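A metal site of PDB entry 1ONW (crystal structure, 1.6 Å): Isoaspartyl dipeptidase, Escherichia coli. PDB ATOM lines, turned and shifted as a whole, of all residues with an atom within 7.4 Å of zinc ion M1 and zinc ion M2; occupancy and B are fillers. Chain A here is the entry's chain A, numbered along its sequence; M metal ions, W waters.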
ATOM      1  N   HIS A  68      -3.472  14.096  -1.116  1.00  0.00           N
ATOM      2  CA  HIS A  68      -3.056  14.609   0.175  1.00  0.00           C
ATOM      3  C   HIS A  68      -3.200  16.102   0.221  1.00  0.00           C
ATOM      4  O   HIS A  68      -2.248  16.837  -0.040  1.00  0.00           O
ATOM      5  CB  HIS A  68      -1.612  14.181   0.485  1.00  0.00           C
ATOM      6  CG  HIS A  68      -1.181  14.440   1.910  1.00  0.00           C
ATOM      7  ND1 HIS A  68      -0.635  13.416   2.678  1.00  0.00           N
ATOM      8  CD2 HIS A  68      -1.169  15.576   2.652  1.00  0.00           C
ATOM      9  CE1 HIS A  68      -0.311  13.911   3.861  1.00  0.00           C
ATOM     10  NE2 HIS A  68      -0.646  15.190   3.858  1.00  0.00           N
ATOM     11  N   VAL A  69      -4.419  16.550   0.518  1.00  0.00           N
ATOM     12  CA  VAL A  69      -4.715  17.968   0.591  1.00  0.00           C
ATOM     13  C   VAL A  69      -5.390  18.341   1.912  1.00  0.00           C
ATOM     14  O   VAL A  69      -6.319  17.690   2.358  1.00  0.00           O
ATOM     15  CB  VAL A  69      -5.650  18.365  -0.565  1.00  0.00           C
ATOM     16  CG1 VAL A  69      -5.787  19.897  -0.640  1.00  0.00           C
ATOM     17  CG2 VAL A  69      -5.115  17.819  -1.891  1.00  0.00           C
ATOM     18  N   HIS A  70      -4.954  19.447   2.519  1.00  0.00           N
ATOM     19  CA  HIS A  70      -5.598  19.918   3.755  1.00  0.00           C
ATOM     20  C   HIS A  70      -6.748  20.845   3.340  1.00  0.00           C
ATOM     21  O   HIS A  70      -6.714  22.085   3.440  1.00  0.00           O
ATOM     22  CB  HIS A  70      -4.562  20.605   4.666  1.00  0.00           C
ATOM     23  CG  HIS A  70      -3.580  19.591   5.118  1.00  0.00           C
ATOM     24  ND1 HIS A  70      -3.735  18.886   6.318  1.00  0.00           N
ATOM     25  CD2 HIS A  70      -2.475  19.115   4.486  1.00  0.00           C
ATOM     26  CE1 HIS A  70      -2.706  18.041   6.410  1.00  0.00           C
ATOM     27  NE2 HIS A  70      -1.953  18.156   5.326  1.00  0.00           N
ATOM     28  N   LEU A 103      -7.536  15.563   4.096  1.00  0.00           N
ATOM     29  CA  LEU A 103      -7.160  14.938   5.349  1.00  0.00           C
ATOM     30  C   LEU A 103      -6.809  16.028   6.356  1.00  0.00           C
ATOM     31  O   LEU A 103      -6.734  17.210   6.022  1.00  0.00           O
ATOM     32  CB  LEU A 103      -6.007  13.893   5.197  1.00  0.00           C
ATOM     33  CG  LEU A 103      -4.894  14.325   4.243  1.00  0.00           C
ATOM     34  CD1 LEU A 103      -4.155  15.506   4.838  1.00  0.00           C
ATOM     35  CD2 LEU A 103      -3.888  13.195   4.019  1.00  0.00           C
ATOM     36  N   LEU A 104      -6.576  15.566   7.580  1.00  0.00           N
ATOM     37  CA  LEU A 104      -6.159  16.416   8.698  1.00  0.00           C
ATOM     38  C   LEU A 104      -4.723  16.040   9.092  1.00  0.00           C
ATOM     39  O   LEU A 104      -4.248  14.955   8.727  1.00  0.00           O
ATOM     40  CB  LEU A 104      -7.067  16.231   9.945  1.00  0.00           C
ATOM     41  CG  LEU A 104      -8.566  16.492   9.734  1.00  0.00           C
ATOM     42  CD1 LEU A 104      -9.284  16.339  11.083  1.00  0.00           C
ATOM     43  CD2 LEU A 104      -8.756  17.936   9.248  1.00  0.00           C
ATOM     44  N   GLY A 105      -4.059  16.870   9.881  1.00  0.00           N
ATOM     45  CA  GLY A 105      -2.682  16.597  10.275  1.00  0.00           C
ATOM     46  C   GLY A 105      -2.460  16.707  11.767  1.00  0.00           C
ATOM     47  O   GLY A 105      -3.076  16.002  12.569  1.00  0.00           O
ATOM     48  N   THR A 106      -1.471  17.518  12.121  1.00  0.00           N
ATOM     49  CA  THR A 106      -1.104  17.709  13.505  1.00  0.00           C
ATOM     50  C   THR A 106      -2.307  18.101  14.366  1.00  0.00           C
ATOM     51  O   THR A 106      -2.563  17.518  15.413  1.00  0.00           O
ATOM     52  CB  THR A 106      -0.024  18.781  13.629  1.00  0.00           C
ATOM     53  OG1 THR A 106       1.005  18.436  12.730  1.00  0.00           O
ATOM     54  CG2 THR A 106       0.516  18.761  15.029  1.00  0.00           C
ATOM     55  N   TYR A 137      -3.153  13.187  12.670  1.00  0.00           N
ATOM     56  CA  TYR A 137      -1.938  12.543  13.195  1.00  0.00           C
ATOM     57  C   TYR A 137      -2.275  11.728  14.423  1.00  0.00           C
ATOM     58  O   TYR A 137      -1.662  10.691  14.684  1.00  0.00           O
ATOM     59  CB  TYR A 137      -0.849  13.527  13.692  1.00  0.00           C
ATOM     60  CG  TYR A 137      -0.040  14.284  12.641  1.00  0.00           C
ATOM     61  CD1 TYR A 137      -0.427  14.359  11.312  1.00  0.00           C
ATOM     62  CD2 TYR A 137       1.132  14.936  13.042  1.00  0.00           C
ATOM     63  CE1 TYR A 137       0.325  15.089  10.384  1.00  0.00           C
ATOM     64  CE2 TYR A 137       1.899  15.669  12.130  1.00  0.00           C
ATOM     65  CZ  TYR A 137       1.487  15.742  10.800  1.00  0.00           C
ATOM     66  OH  TYR A 137       2.203  16.482   9.902  1.00  0.00           O
ATOM     67  N   KCX A 162      -5.980   8.343   8.441  1.00  0.00           N
ATOM     68  CA  KCX A 162      -4.716   9.038   8.474  1.00  0.00           C
ATOM     69  CB  KCX A 162      -4.954  10.549   8.238  1.00  0.00           C
ATOM     70  CG  KCX A 162      -3.756  11.430   8.581  1.00  0.00           C
ATOM     71  CD  KCX A 162      -2.625  11.256   7.565  1.00  0.00           C
ATOM     72  CE  KCX A 162      -1.453  12.203   7.787  1.00  0.00           C
ATOM     73  NZ  KCX A 162      -1.875  13.575   7.503  1.00  0.00           N
ATOM     74  C   KCX A 162      -4.087   8.868   9.860  1.00  0.00           C
ATOM     75  O   KCX A 162      -4.804   8.650  10.860  1.00  0.00           O
ATOM     76  CX  KCX A 162      -0.736  14.320   7.047  1.00  0.00           C
ATOM     77  OQ1 KCX A 162       0.339  13.809   6.781  1.00  0.00           O
ATOM     78  OQ2 KCX A 162      -1.011  15.586   6.937  1.00  0.00           O
ATOM     79  N   CYS A 163      -2.757   8.959   9.938  1.00  0.00           N
ATOM     80  CA  CYS A 163      -2.005   8.878  11.187  1.00  0.00           C
ATOM     81  C   CYS A 163      -0.596   9.449  10.994  1.00  0.00           C
ATOM     82  O   CYS A 163      -0.174   9.737   9.896  1.00  0.00           O
ATOM     83  CB  CYS A 163      -1.958   7.459  11.792  1.00  0.00           C
ATOM     84  SG  CYS A 163      -0.766   6.311  11.021  1.00  0.00           S
ATOM     85  N   ALA A 164       0.131   9.611  12.083  1.00  0.00           N
ATOM     86  CA  ALA A 164       1.509  10.074  12.024  1.00  0.00           C
ATOM     87  C   ALA A 164       2.364   9.107  12.819  1.00  0.00           C
ATOM     88  O   ALA A 164       1.992   8.679  13.911  1.00  0.00           O
ATOM     89  CB  ALA A 164       1.695  11.458  12.626  1.00  0.00           C
ATOM     90  N   ASP A 167       7.592  10.673  14.121  1.00  0.00           N
ATOM     91  CA  ASP A 167       7.560  12.112  14.015  1.00  0.00           C
ATOM     92  C   ASP A 167       7.391  12.751  15.390  1.00  0.00           C
ATOM     93  O   ASP A 167       6.607  12.264  16.195  1.00  0.00           O
ATOM     94  CB  ASP A 167       6.393  12.492  13.093  1.00  0.00           C
ATOM     95  CG  ASP A 167       6.316  13.974  12.894  1.00  0.00           C
ATOM     96  OD1 ASP A 167       5.843  14.778  13.681  1.00  0.00           O
ATOM     97  OD2 ASP A 167       6.791  14.309  11.747  1.00  0.00           O
ATOM     98  N   ARG A 169       5.727  15.022  16.293  1.00  0.00           N
ATOM     99  CA  ARG A 169       4.351  15.497  16.508  1.00  0.00           C
ATOM    100  C   ARG A 169       3.361  14.356  16.576  1.00  0.00           C
ATOM    101  O   ARG A 169       2.162  14.591  16.499  1.00  0.00           O
ATOM    102  CB  ARG A 169       3.862  16.478  15.454  1.00  0.00           C
ATOM    103  CG  ARG A 169       4.616  17.788  15.422  1.00  0.00           C
ATOM    104  CD  ARG A 169       4.609  18.389  14.016  1.00  0.00           C
ATOM    105  NE  ARG A 169       5.294  17.506  13.073  1.00  0.00           N
ATOM    106  CZ  ARG A 169       5.448  17.768  11.774  1.00  0.00           C
ATOM    107  NH1 ARG A 169       4.970  18.872  11.199  1.00  0.00           N
ATOM    108  NH2 ARG A 169       6.089  16.889  11.016  1.00  0.00           N
ATOM    109  N   PHE A 200       0.315   6.974   6.298  1.00  0.00           N
ATOM    110  CA  PHE A 200       1.226   7.335   7.343  1.00  0.00           C
ATOM    111  C   PHE A 200       2.065   8.574   7.106  1.00  0.00           C
ATOM    112  O   PHE A 200       2.969   8.573   6.268  1.00  0.00           O
ATOM    113  CB  PHE A 200       2.236   6.215   7.568  1.00  0.00           C
ATOM    114  CG  PHE A 200       1.580   4.930   7.919  1.00  0.00           C
ATOM    115  CD1 PHE A 200       1.086   4.105   6.910  1.00  0.00           C
ATOM    116  CD2 PHE A 200       1.485   4.536   9.253  1.00  0.00           C
ATOM    117  CE1 PHE A 200       0.491   2.894   7.243  1.00  0.00           C
ATOM    118  CE2 PHE A 200       0.890   3.321   9.600  1.00  0.00           C
ATOM    119  CZ  PHE A 200       0.404   2.491   8.589  1.00  0.00           C
ATOM    120  N   HIS A 201       1.795   9.629   7.866  1.00  0.00           N
ATOM    121  CA  HIS A 201       2.599  10.819   7.753  1.00  0.00           C
ATOM    122  C   HIS A 201       3.902  10.399   8.370  1.00  0.00           C
ATOM    123  O   HIS A 201       3.903   9.932   9.507  1.00  0.00           O
ATOM    124  CB  HIS A 201       2.042  11.980   8.592  1.00  0.00           C
ATOM    125  CG  HIS A 201       3.105  12.970   8.949  1.00  0.00           C
ATOM    126  ND1 HIS A 201       3.299  14.144   8.224  1.00  0.00           N
ATOM    127  CD2 HIS A 201       4.029  12.947   9.943  1.00  0.00           C
ATOM    128  CE1 HIS A 201       4.302  14.810   8.770  1.00  0.00           C
ATOM    129  NE2 HIS A 201       4.767  14.121   9.814  1.00  0.00           N
ATOM    130  N   MET A 202       4.986  10.500   7.620  1.00  0.00           N
ATOM    131  CA  MET A 202       6.289  10.124   8.140  1.00  0.00           C
ATOM    132  C   MET A 202       7.035  11.360   8.641  1.00  0.00           C
ATOM    133  O   MET A 202       6.984  12.404   7.988  1.00  0.00           O
ATOM    134  CB  MET A 202       7.188   9.448   7.082  1.00  0.00           C
ATOM    135  CG  MET A 202       6.526   8.250   6.456  1.00  0.00           C
ATOM    136  SD  MET A 202       6.098   6.959   7.651  1.00  0.00           S
ATOM    137  CE  MET A 202       7.668   6.773   8.568  1.00  0.00           C
ATOM    138  N   THR A 229       3.856   8.401   3.459  1.00  0.00           N
ATOM    139  CA  THR A 229       3.929   9.623   2.655  1.00  0.00           C
ATOM    140  C   THR A 229       5.053  10.502   3.149  1.00  0.00           C
ATOM    141  O   THR A 229       5.568  10.251   4.256  1.00  0.00           O
ATOM    142  CB  THR A 229       2.545  10.317   2.487  1.00  0.00           C
ATOM    143  OG1 THR A 229       2.681  11.370   1.548  1.00  0.00           O
ATOM    144  CG2 THR A 229       1.946  10.786   3.821  1.00  0.00           C
ATOM    145  N   HIS A 230       5.488  11.483   2.353  1.00  0.00           N
ATOM    146  CA  HIS A 230       6.610  12.345   2.730  1.00  0.00           C
ATOM    147  C   HIS A 230       7.886  11.517   2.707  1.00  0.00           C
ATOM    148  O   HIS A 230       8.857  11.796   3.401  1.00  0.00           O
ATOM    149  CB  HIS A 230       6.476  12.910   4.158  1.00  0.00           C
ATOM    150  CG  HIS A 230       5.161  13.552   4.408  1.00  0.00           C
ATOM    151  ND1 HIS A 230       4.534  14.320   3.456  1.00  0.00           N
ATOM    152  CD2 HIS A 230       4.383  13.552   5.521  1.00  0.00           C
ATOM    153  CE1 HIS A 230       3.408  14.764   3.972  1.00  0.00           C
ATOM    154  NE2 HIS A 230       3.293  14.313   5.211  1.00  0.00           N
ATOM    155  N   ARG A 233      11.380  13.098   2.425  1.00  0.00           N
ATOM    156  CA  ARG A 233      11.758  14.042   3.460  1.00  0.00           C
ATOM    157  C   ARG A 233      13.153  13.846   4.021  1.00  0.00           C
ATOM    158  O   ARG A 233      13.763  14.785   4.545  1.00  0.00           O
ATOM    159  CB  ARG A 233      10.708  14.114   4.559  1.00  0.00           C
ATOM    160  CG  ARG A 233      10.764  12.927   5.508  1.00  0.00           C
ATOM    161  CD  ARG A 233       9.849  13.100   6.700  1.00  0.00           C
ATOM    162  NE  ARG A 233       9.993  14.435   7.268  1.00  0.00           N
ATOM    163  CZ  ARG A 233       9.039  15.346   7.395  1.00  0.00           C
ATOM    164  NH1 ARG A 233       7.757  15.127   7.069  1.00  0.00           N
ATOM    165  NH2 ARG A 233       9.382  16.511   7.919  1.00  0.00           N
ATOM    166  N   THR A 254       6.088  13.504  -1.775  1.00  0.00           N
ATOM    167  CA  THR A 254       5.440  14.813  -1.659  1.00  0.00           C
ATOM    168  C   THR A 254       6.045  15.862  -2.589  1.00  0.00           C
ATOM    169  O   THR A 254       7.208  16.186  -2.481  1.00  0.00           O
ATOM    170  CB  THR A 254       5.406  15.275  -0.178  1.00  0.00           C
ATOM    171  OG1 THR A 254       4.864  14.245   0.620  1.00  0.00           O
ATOM    172  CG2 THR A 254       4.598  16.560  -0.041  1.00  0.00           C
ATOM    173  N   SER A 284       0.502  16.566  -3.094  1.00  0.00           N
ATOM    174  CA  SER A 284       1.085  17.874  -2.838  1.00  0.00           C
ATOM    175  C   SER A 284       1.261  18.271  -1.404  1.00  0.00           C
ATOM    176  O   SER A 284       2.156  19.066  -1.091  1.00  0.00           O
ATOM    177  CB  SER A 284       0.201  18.946  -3.497  1.00  0.00           C
ATOM    178  OG  SER A 284      -1.095  18.951  -2.887  1.00  0.00           O
ATOM    179  N   ASP A 285       0.360  17.809  -0.546  1.00  0.00           N
ATOM    180  CA  ASP A 285       0.342  18.259   0.844  1.00  0.00           C
ATOM    181  C   ASP A 285      -0.089  19.739   0.848  1.00  0.00           C
ATOM    182  O   ASP A 285       0.270  20.537   1.722  1.00  0.00           O
ATOM    183  CB  ASP A 285       1.630  18.070   1.632  1.00  0.00           C
ATOM    184  CG  ASP A 285       1.295  18.089   3.095  1.00  0.00           C
ATOM    185  OD1 ASP A 285       0.155  18.074   3.476  1.00  0.00           O
ATOM    186  OD2 ASP A 285       2.336  18.135   3.895  1.00  0.00           O
ATOM    187  N   GLY A 286      -0.863  20.086  -0.175  1.00  0.00           N
ATOM    188  CA  GLY A 286      -1.344  21.424  -0.413  1.00  0.00           C
ATOM    189  C   GLY A 286      -2.260  21.957   0.665  1.00  0.00           C
ATOM    190  O   GLY A 286      -3.039  21.244   1.300  1.00  0.00           O
ATOM    191  N   GLY A 288      -1.371  23.087   3.343  1.00  0.00           N
ATOM    192  CA  GLY A 288      -0.821  22.959   4.649  1.00  0.00           C
ATOM    193  C   GLY A 288       0.013  24.223   4.903  1.00  0.00           C
ATOM    194  O   GLY A 288      -0.019  25.187   4.106  1.00  0.00           O
HETATM  195 ZN    ZN M   1       2.090  15.003   6.801  1.00  0.00          ZN
HETATM  196 ZN    ZN M   2      -0.419  16.742   5.342  1.00  0.00          ZN
HETATM  197  O   HOH W   1       1.338  17.089   6.450  1.00  0.00           O
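CD1 of Leu 103 touches zinc ion M2 (3.97 Å). Within 4 Å of zinc ion M2: His 68, His 70, Leu 103, KCX 162 and Asp 285. The nearest printed residue that does not touch zinc ion M2 is His 230 (4.4 Å).
Zinc ion M1 is bound by ND1 of His 201 (2.1 Å), NE2 of His 230 (2.1 Å), OQ1 of KCX 162 (2.1 Å) and water W1 (2.2 Å).
N of His 70 lies within hydrogen-bond range of O of Gly 286. N of Tyr 137 is in hydrogen-bond range of O of Gly 105 (2.8 Å). The side-chain carboxylate of Asp 167 sits at hydrogen-bond distance from a ring nitrogen (NE2) of His 201, 2.8 Å away. O of Tyr 137 lies within hydrogen-bond range of N of Ala 164 (3.3 Å). N of Leu 103 sits at hydrogen-bond distance from O of Val 69, at 3.0 Å. A ring nitrogen (ND1) of His 230 is in hydrogen-bond range of the side-chain hydroxyl (OG1) of Thr 254. The guanidinium group (NH2) of Arg 169 lies within hydrogen-bond range of a ring nitrogen (NE2) of His 201 (3.3 Å). N of His 201 lies within hydrogen-bond range of O of Cys 163, at 2.8 Å.
Zinc ion M2 is bound by OQ2 of KCX 162 (2.1 Å), a ring nitrogen (NE2) of His 70 (2.1 Å), water W1 (2.1 Å), a ring nitrogen (NE2) of His 68 (2.2 Å) and the side-chain carboxylate (OD1) of Asp 285 (2.4 Å). Zinc ion M2 has five donor atoms within binding distance.
Tyr 137 touches zinc ion M1 (OH to ZN, 3.4 Å). Five residues have an atom within 4 Å of zinc ion M1: His 68, Tyr 137, KCX 162, His 201 and His 230. Along chain A the residues within 4 Å of zinc ion M1 span positions 68 to 230. The nearest printed residue that does not touch zinc ion M1 is Asp 285 (4.3 Å).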
